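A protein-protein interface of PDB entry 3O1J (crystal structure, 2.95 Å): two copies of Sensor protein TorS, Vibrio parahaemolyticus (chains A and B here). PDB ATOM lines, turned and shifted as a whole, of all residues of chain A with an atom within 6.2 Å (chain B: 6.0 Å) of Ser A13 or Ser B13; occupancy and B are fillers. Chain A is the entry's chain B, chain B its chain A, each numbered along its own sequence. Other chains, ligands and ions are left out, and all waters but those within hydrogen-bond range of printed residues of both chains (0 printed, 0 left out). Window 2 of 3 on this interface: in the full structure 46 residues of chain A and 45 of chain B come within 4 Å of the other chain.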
ATOM      1  N   GLU A   8      27.585 -20.675   8.774  1.00  0.00           N
ATOM      2  CA  GLU A   8      28.469 -19.648   9.305  1.00  0.00           C
ATOM      3  C   GLU A   8      27.965 -18.224   9.115  1.00  0.00           C
ATOM      4  O   GLU A   8      28.079 -17.407  10.024  1.00  0.00           O
ATOM      5  CB  GLU A   8      29.864 -19.796   8.693  1.00  0.00           C
ATOM      6  CG  GLU A   8      30.964 -19.877   9.743  1.00  0.00           C
ATOM      7  CD  GLU A   8      30.736 -20.997  10.755  1.00  0.00           C
ATOM      8  OE1 GLU A   8      31.457 -21.044  11.778  1.00  0.00           O
ATOM      9  OE2 GLU A   8      29.839 -21.836  10.524  1.00  0.00           O
ATOM     10  N   ALA A   9      27.408 -17.925   7.946  1.00  0.00           N
ATOM     11  CA  ALA A   9      26.897 -16.585   7.671  1.00  0.00           C
ATOM     12  C   ALA A   9      25.585 -16.297   8.408  1.00  0.00           C
ATOM     13  O   ALA A   9      25.150 -15.145   8.485  1.00  0.00           O
ATOM     14  CB  ALA A   9      26.716 -16.391   6.172  1.00  0.00           C
ATOM     15  N   ARG A  10      24.950 -17.342   8.935  1.00  0.00           N
ATOM     16  CA  ARG A  10      23.707 -17.174   9.686  1.00  0.00           C
ATOM     17  C   ARG A  10      24.127 -16.890  11.114  1.00  0.00           C
ATOM     18  O   ARG A  10      23.342 -16.423  11.931  1.00  0.00           O
ATOM     19  CB  ARG A  10      22.843 -18.441   9.631  1.00  0.00           C
ATOM     20  CG  ARG A  10      21.519 -18.277   8.850  1.00  0.00           C
ATOM     21  CD  ARG A  10      20.747 -19.604   8.688  1.00  0.00           C
ATOM     22  NE  ARG A  10      19.842 -19.919   9.799  1.00  0.00           N
ATOM     23  CZ  ARG A  10      20.198 -20.048  11.078  1.00  0.00           C
ATOM     24  NH1 ARG A  10      21.460 -19.891  11.459  1.00  0.00           N
ATOM     25  NH2 ARG A  10      19.279 -20.343  11.988  1.00  0.00           N
ATOM     26  N   GLN A  11      25.386 -17.186  11.398  1.00  0.00           N
ATOM     27  CA  GLN A  11      25.950 -16.941  12.709  1.00  0.00           C
ATOM     28  C   GLN A  11      26.465 -15.506  12.737  1.00  0.00           C
ATOM     29  O   GLN A  11      26.477 -14.857  13.779  1.00  0.00           O
ATOM     30  CB  GLN A  11      27.094 -17.920  12.975  1.00  0.00           C
ATOM     31  CG  GLN A  11      26.682 -19.144  13.767  1.00  0.00           C
ATOM     32  CD  GLN A  11      26.281 -18.800  15.199  1.00  0.00           C
ATOM     33  OE1 GLN A  11      25.999 -19.689  16.008  1.00  0.00           O
ATOM     34  NE2 GLN A  11      26.257 -17.505  15.518  1.00  0.00           N
ATOM     35  N   VAL A  12      26.878 -15.021  11.570  1.00  0.00           N
ATOM     36  CA  VAL A  12      27.399 -13.668  11.417  1.00  0.00           C
ATOM     37  C   VAL A  12      26.265 -12.655  11.378  1.00  0.00           C
ATOM     38  O   VAL A  12      26.272 -11.673  12.119  1.00  0.00           O
ATOM     39  CB  VAL A  12      28.226 -13.544  10.118  1.00  0.00           C
ATOM     40  CG1 VAL A  12      28.562 -12.088   9.838  1.00  0.00           C
ATOM     41  CG2 VAL A  12      29.495 -14.372  10.240  1.00  0.00           C
ATOM     42  N   SER A  13      25.294 -12.900  10.504  1.00  0.00           N
ATOM     43  CA  SER A  13      24.140 -12.018  10.359  1.00  0.00           C
ATOM     44  C   SER A  13      23.408 -11.898  11.696  1.00  0.00           C
ATOM     45  O   SER A  13      23.003 -10.807  12.101  1.00  0.00           O
ATOM     46  CB  SER A  13      23.190 -12.577   9.288  1.00  0.00           C
ATOM     47  OG  SER A  13      22.192 -11.638   8.928  1.00  0.00           O
ATOM     48  N   GLU A  14      23.256 -13.030  12.377  1.00  0.00           N
ATOM     49  CA  GLU A  14      22.578 -13.078  13.666  1.00  0.00           C
ATOM     50  C   GLU A  14      23.387 -12.348  14.760  1.00  0.00           C
ATOM     51  O   GLU A  14      22.830 -11.541  15.509  1.00  0.00           O
ATOM     52  CB  GLU A  14      22.317 -14.546  14.051  1.00  0.00           C
ATOM     53  CG  GLU A  14      21.184 -14.795  15.063  1.00  0.00           C
ATOM     54  CD  GLU A  14      21.545 -14.384  16.499  1.00  0.00           C
ATOM     55  OE1 GLU A  14      22.625 -14.803  16.993  1.00  0.00           O
ATOM     56  OE2 GLU A  14      20.744 -13.652  17.135  1.00  0.00           O
ATOM     57  N   LEU A  15      24.693 -12.609  14.854  1.00  0.00           N
ATOM     58  CA  LEU A  15      25.521 -11.945  15.868  1.00  0.00           C
ATOM     59  C   LEU A  15      25.682 -10.448  15.624  1.00  0.00           C
ATOM     60  O   LEU A  15      25.897  -9.694  16.566  1.00  0.00           O
ATOM     61  CB  LEU A  15      26.906 -12.594  15.969  1.00  0.00           C
ATOM     62  CG  LEU A  15      27.063 -13.621  17.093  1.00  0.00           C
ATOM     63  CD1 LEU A  15      28.482 -14.165  17.123  1.00  0.00           C
ATOM     64  CD2 LEU A  15      26.730 -12.963  18.413  1.00  0.00           C
ATOM     65  N   SER A  16      25.586 -10.021  14.368  1.00  0.00           N
ATOM     66  CA  SER A  16      25.696  -8.600  14.050  1.00  0.00           C
ATOM     67  C   SER A  16      24.584  -7.843  14.764  1.00  0.00           C
ATOM     68  O   SER A  16      24.838  -6.817  15.389  1.00  0.00           O
ATOM     69  CB  SER A  16      25.572  -8.356  12.546  1.00  0.00           C
ATOM     70  OG  SER A  16      26.628  -8.963  11.834  1.00  0.00           O
ATOM     71  N   THR A  17      23.353  -8.346  14.672  1.00  0.00           N
ATOM     72  CA  THR A  17      22.222  -7.692  15.325  1.00  0.00           C
ATOM     73  C   THR A  17      22.488  -7.561  16.819  1.00  0.00           C
ATOM     74  O   THR A  17      22.490  -6.454  17.360  1.00  0.00           O
ATOM     75  CB  THR A  17      20.913  -8.472  15.140  1.00  0.00           C
ATOM     76  OG1 THR A  17      20.741  -8.798  13.761  1.00  0.00           O
ATOM     77  CG2 THR A  17      19.734  -7.618  15.570  1.00  0.00           C
ATOM     78  N   ARG A  18      22.717  -8.691  17.482  1.00  0.00           N
ATOM     79  CA  ARG A  18      22.993  -8.692  18.913  1.00  0.00           C
ATOM     80  C   ARG A  18      24.120  -7.728  19.309  1.00  0.00           C
ATOM     81  O   ARG A  18      24.165  -7.266  20.446  1.00  0.00           O
ATOM     82  CB  ARG A  18      23.331 -10.110  19.378  1.00  0.00           C
ATOM     83  CG  ARG A  18      22.147 -11.084  19.384  1.00  0.00           C
ATOM     84  CD  ARG A  18      22.624 -12.531  19.544  1.00  0.00           C
ATOM     85  NE  ARG A  18      23.579 -12.679  20.647  1.00  0.00           N
ATOM     86  CZ  ARG A  18      24.405 -13.715  20.799  1.00  0.00           C
ATOM     87  NH1 ARG A  18      24.395 -14.707  19.913  1.00  0.00           N
ATOM     88  NH2 ARG A  18      25.250 -13.752  21.829  1.00  0.00           N
ATOM     89  N   LEU A  49      32.107 -13.265  16.701  1.00  0.00           N
ATOM     90  CA  LEU A  49      31.922 -12.781  15.339  1.00  0.00           C
ATOM     91  C   LEU A  49      33.177 -13.018  14.521  1.00  0.00           C
ATOM     92  O   LEU A  49      33.106 -13.363  13.338  1.00  0.00           O
ATOM     93  CB  LEU A  49      31.615 -11.288  15.314  1.00  0.00           C
ATOM     94  CG  LEU A  49      31.347 -10.838  13.877  1.00  0.00           C
ATOM     95  CD1 LEU A  49      30.005 -11.389  13.451  1.00  0.00           C
ATOM     96  CD2 LEU A  49      31.350  -9.334  13.757  1.00  0.00           C
ATOM     97  N   ASN A 261      27.813  -7.510   6.247  1.00  0.00           N
ATOM     98  CA  ASN A 261      26.869  -8.530   5.790  1.00  0.00           C
ATOM     99  C   ASN A 261      26.639  -8.552   4.288  1.00  0.00           C
ATOM    100  O   ASN A 261      26.403  -9.614   3.713  1.00  0.00           O
ATOM    101  CB  ASN A 261      25.546  -8.411   6.538  1.00  0.00           C
ATOM    102  CG  ASN A 261      25.640  -8.972   7.943  1.00  0.00           C
ATOM    103  OD1 ASN A 261      26.183  -8.331   8.845  1.00  0.00           O
ATOM    104  ND2 ASN A 261      25.141 -10.189   8.129  1.00  0.00           N
ATOM    105  N   VAL A 264      29.516 -10.588   3.371  1.00  0.00           N
ATOM    106  CA  VAL A 264      29.435 -11.978   3.808  1.00  0.00           C
ATOM    107  C   VAL A 264      28.354 -12.723   3.043  1.00  0.00           C
ATOM    108  O   VAL A 264      28.229 -13.939   3.175  1.00  0.00           O
ATOM    109  CB  VAL A 264      29.136 -12.129   5.317  1.00  0.00           C
ATOM    110  CG1 VAL A 264      29.917 -11.100   6.106  1.00  0.00           C
ATOM    111  CG2 VAL A 264      27.640 -12.022   5.577  1.00  0.00           C
ATOM    112  N   GLU B   8      14.871 -13.817   0.192  1.00  0.00           N
ATOM    113  CA  GLU B   8      13.954 -12.864   0.809  1.00  0.00           C
ATOM    114  C   GLU B   8      14.404 -12.444   2.209  1.00  0.00           C
ATOM    115  O   GLU B   8      14.192 -11.302   2.609  1.00  0.00           O
ATOM    116  CB  GLU B   8      12.544 -13.463   0.867  1.00  0.00           C
ATOM    117  CG  GLU B   8      11.436 -12.498   0.449  1.00  0.00           C
ATOM    118  CD  GLU B   8      11.378 -12.259  -1.057  1.00  0.00           C
ATOM    119  OE1 GLU B   8      10.627 -11.355  -1.499  1.00  0.00           O
ATOM    120  OE2 GLU B   8      12.076 -12.982  -1.802  1.00  0.00           O
ATOM    121  N   ALA B   9      15.015 -13.363   2.954  1.00  0.00           N
ATOM    122  CA  ALA B   9      15.494 -13.054   4.300  1.00  0.00           C
ATOM    123  C   ALA B   9      16.650 -12.062   4.195  1.00  0.00           C
ATOM    124  O   ALA B   9      16.857 -11.238   5.085  1.00  0.00           O
ATOM    125  CB  ALA B   9      15.946 -14.323   5.000  1.00  0.00           C
ATOM    126  N   ARG B  10      17.401 -12.153   3.099  1.00  0.00           N
ATOM    127  CA  ARG B  10      18.517 -11.246   2.845  1.00  0.00           C
ATOM    128  C   ARG B  10      17.904  -9.851   2.744  1.00  0.00           C
ATOM    129  O   ARG B  10      18.539  -8.847   3.051  1.00  0.00           O
ATOM    130  CB  ARG B  10      19.198 -11.579   1.512  1.00  0.00           C
ATOM    131  CG  ARG B  10      20.635 -12.093   1.588  1.00  0.00           C
ATOM    132  CD  ARG B  10      20.684 -13.615   1.712  1.00  0.00           C
ATOM    133  NE  ARG B  10      21.951 -14.202   1.260  1.00  0.00           N
ATOM    134  CZ  ARG B  10      22.472 -14.024   0.049  1.00  0.00           C
ATOM    135  NH1 ARG B  10      21.846 -13.266  -0.845  1.00  0.00           N
ATOM    136  NH2 ARG B  10      23.614 -14.618  -0.272  1.00  0.00           N
ATOM    137  N   GLN B  11      16.658  -9.810   2.289  1.00  0.00           N
ATOM    138  CA  GLN B  11      15.916  -8.571   2.133  1.00  0.00           C
ATOM    139  C   GLN B  11      15.542  -8.027   3.505  1.00  0.00           C
ATOM    140  O   GLN B  11      15.582  -6.820   3.745  1.00  0.00           O
ATOM    141  CB  GLN B  11      14.635  -8.834   1.347  1.00  0.00           C
ATOM    142  CG  GLN B  11      14.826  -9.191  -0.111  1.00  0.00           C
ATOM    143  CD  GLN B  11      15.035  -7.965  -0.971  1.00  0.00           C
ATOM    144  OE1 GLN B  11      14.865  -8.018  -2.189  1.00  0.00           O
ATOM    145  NE2 GLN B  11      15.408  -6.848  -0.341  1.00  0.00           N
ATOM    146  N   VAL B  12      15.160  -8.939   4.392  1.00  0.00           N
ATOM    147  CA  VAL B  12      14.753  -8.595   5.747  1.00  0.00           C
ATOM    148  C   VAL B  12      15.915  -8.131   6.618  1.00  0.00           C
ATOM    149  O   VAL B  12      15.900  -7.005   7.114  1.00  0.00           O
ATOM    150  CB  VAL B  12      14.044  -9.792   6.414  1.00  0.00           C
ATOM    151  CG1 VAL B  12      13.914  -9.573   7.907  1.00  0.00           C
ATOM    152  CG2 VAL B  12      12.677  -9.978   5.788  1.00  0.00           C
ATOM    153  N   SER B  13      16.916  -8.989   6.808  1.00  0.00           N
ATOM    154  CA  SER B  13      18.073  -8.625   7.622  1.00  0.00           C
ATOM    155  C   SER B  13      18.658  -7.294   7.154  1.00  0.00           C
ATOM    156  O   SER B  13      19.194  -6.524   7.948  1.00  0.00           O
ATOM    157  CB  SER B  13      19.148  -9.710   7.541  1.00  0.00           C
ATOM    158  OG  SER B  13      20.299  -9.344   8.285  1.00  0.00           O
ATOM    159  N   GLU B  14      18.535  -7.024   5.861  1.00  0.00           N
ATOM    160  CA  GLU B  14      19.053  -5.794   5.285  1.00  0.00           C
ATOM    161  C   GLU B  14      18.154  -4.600   5.621  1.00  0.00           C
ATOM    162  O   GLU B  14      18.593  -3.641   6.259  1.00  0.00           O
ATOM    163  CB  GLU B  14      19.176  -5.946   3.766  1.00  0.00           C
ATOM    164  CG  GLU B  14      20.274  -5.097   3.143  1.00  0.00           C
ATOM    165  CD  GLU B  14      20.186  -3.639   3.557  1.00  0.00           C
ATOM    166  OE1 GLU B  14      19.120  -3.032   3.311  1.00  0.00           O
ATOM    167  OE2 GLU B  14      21.172  -3.108   4.129  1.00  0.00           O
ATOM    168  N   LEU B  15      16.899  -4.654   5.184  1.00  0.00           N
ATOM    169  CA  LEU B  15      15.954  -3.576   5.453  1.00  0.00           C
ATOM    170  C   LEU B  15      15.840  -3.289   6.949  1.00  0.00           C
ATOM    171  O   LEU B  15      15.569  -2.156   7.341  1.00  0.00           O
ATOM    172  CB  LEU B  15      14.577  -3.913   4.870  1.00  0.00           C
ATOM    173  CG  LEU B  15      14.336  -3.524   3.405  1.00  0.00           C
ATOM    174  CD1 LEU B  15      13.150  -4.286   2.849  1.00  0.00           C
ATOM    175  CD2 LEU B  15      14.094  -2.024   3.305  1.00  0.00           C
ATOM    176  N   SER B  16      16.043  -4.307   7.782  1.00  0.00           N
ATOM    177  CA  SER B  16      15.982  -4.117   9.231  1.00  0.00           C
ATOM    178  C   SER B  16      16.984  -3.035   9.629  1.00  0.00           C
ATOM    179  O   SER B  16      16.620  -2.031  10.243  1.00  0.00           O
ATOM    180  CB  SER B  16      16.325  -5.416   9.971  1.00  0.00           C
ATOM    181  OG  SER B  16      15.309  -6.390   9.825  1.00  0.00           O
ATOM    182  N   THR B  17      18.251  -3.249   9.271  1.00  0.00           N
ATOM    183  CA  THR B  17      19.320  -2.306   9.575  1.00  0.00           C
ATOM    184  C   THR B  17      18.963  -0.901   9.101  1.00  0.00           C
ATOM    185  O   THR B  17      19.164   0.062   9.829  1.00  0.00           O
ATOM    186  CB  THR B  17      20.646  -2.765   8.933  1.00  0.00           C
ATOM    187  OG1 THR B  17      21.047  -4.002   9.533  1.00  0.00           O
ATOM    188  CG2 THR B  17      21.740  -1.740   9.145  1.00  0.00           C
ATOM    189  N   ARG B  18      18.424  -0.779   7.894  1.00  0.00           N
ATOM    190  CA  ARG B  18      18.037   0.531   7.376  1.00  0.00           C
ATOM    191  C   ARG B  18      16.940   1.180   8.232  1.00  0.00           C
ATOM    192  O   ARG B  18      16.911   2.403   8.408  1.00  0.00           O
ATOM    193  CB  ARG B  18      17.575   0.401   5.920  1.00  0.00           C
ATOM    194  CG  ARG B  18      18.718   0.484   4.907  1.00  0.00           C
ATOM    195  CD  ARG B  18      18.410  -0.254   3.599  1.00  0.00           C
ATOM    196  NE  ARG B  18      17.213   0.230   2.906  1.00  0.00           N
ATOM    197  CZ  ARG B  18      16.652  -0.382   1.862  1.00  0.00           C
ATOM    198  NH1 ARG B  18      17.177  -1.507   1.383  1.00  0.00           N
ATOM    199  NH2 ARG B  18      15.561   0.126   1.294  1.00  0.00           N
ATOM    200  N   ASN B 261      14.867 -11.454  13.364  1.00  0.00           N
ATOM    201  CA  ASN B 261      15.818 -12.171  12.518  1.00  0.00           C
ATOM    202  C   ASN B 261      16.035 -13.606  12.967  1.00  0.00           C
ATOM    203  O   ASN B 261      15.996 -14.522  12.151  1.00  0.00           O
ATOM    204  CB  ASN B 261      17.150 -11.435  12.480  1.00  0.00           C
ATOM    205  CG  ASN B 261      17.251 -10.499  11.300  1.00  0.00           C
ATOM    206  OD1 ASN B 261      16.377  -9.642  11.086  1.00  0.00           O
ATOM    207  ND2 ASN B 261      18.319 -10.654  10.518  1.00  0.00           N
ATOM    208  N   VAL B 264      13.229 -15.351  11.475  1.00  0.00           N
ATOM    209  CA  VAL B 264      13.187 -15.485  10.021  1.00  0.00           C
ATOM    210  C   VAL B 264      14.266 -16.471   9.600  1.00  0.00           C
ATOM    211  O   VAL B 264      14.282 -16.935   8.463  1.00  0.00           O
ATOM    212  CB  VAL B 264      13.424 -14.150   9.261  1.00  0.00           C
ATOM    213  CG1 VAL B 264      12.649 -13.027   9.927  1.00  0.00           C
ATOM    214  CG2 VAL B 264      14.914 -13.844   9.164  1.00  0.00           C
ATOM    215  N   ASN B 265      15.182 -16.782  10.512  1.00  0.00           N
ATOM    216  CA  ASN B 265      16.232 -17.746  10.214  1.00  0.00           C
ATOM    217  C   ASN B 265      15.715 -19.152  10.515  1.00  0.00           C
ATOM    218  O   ASN B 265      15.857 -20.043   9.680  1.00  0.00           O
ATOM    219  CB  ASN B 265      17.504 -17.457  11.021  1.00  0.00           C
ATOM    220  CG  ASN B 265      18.369 -16.369  10.389  1.00  0.00           C
ATOM    221  OD1 ASN B 265      18.122 -15.925   9.261  1.00  0.00           O
ATOM    222  ND2 ASN B 265      19.399 -15.944  11.116  1.00  0.00           N
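The side-chain hydroxyl (OG) of Ser A13 is in hydrogen-bond range of the side-chain hydroxyl (OG) of Ser B13 (3.0 Å).
OG of Ser A13 lies close to ND2 of Asn A261 (3.4 Å). The side-chain amide nitrogen (ND2) of Asn B261 lies close to the side-chain hydroxyl (OG) of Ser B13. The backbone carbonyl oxygen (O) of Ser A13 lies within hydrogen-bond range of the side-chain hydroxyl (OG1) of Thr A17, at 3.5 Å.
Among the printed residues, merely in contact across the chains: Arg A10 with Asn B265.
Ser A13 touches one residue of chain B. Of the printed residues of chain A, Ser B13 touches Ser A13 (3.0 Å). Of the printed residues of chain A, Asn B265 touches Arg A10. Of the printed residues of chain B, Arg A10 touches Asn B265. Leu B15 touches none of the printed residues of chain A. The nearest residue of chain B that does not touch Ser A13 is Asn B261 (4.3 Å). The nearest residue of chain A that does not touch Ser B13 is Asn A261 (4.9 Å).
Printed residues of chain A that touch a printed residue of chain B: Arg A10 and Ser A13. Of the 14 printed residues of chain B, 2 touch a printed residue of chain A. Among the printed residues, 2 pairs touch across the chains.
Ser B13 touches its own counterpart, Ser A13. Of the 2 pairs that touch across the chains among the printed residues, 1 has its exchanged pair printed and touching as well.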
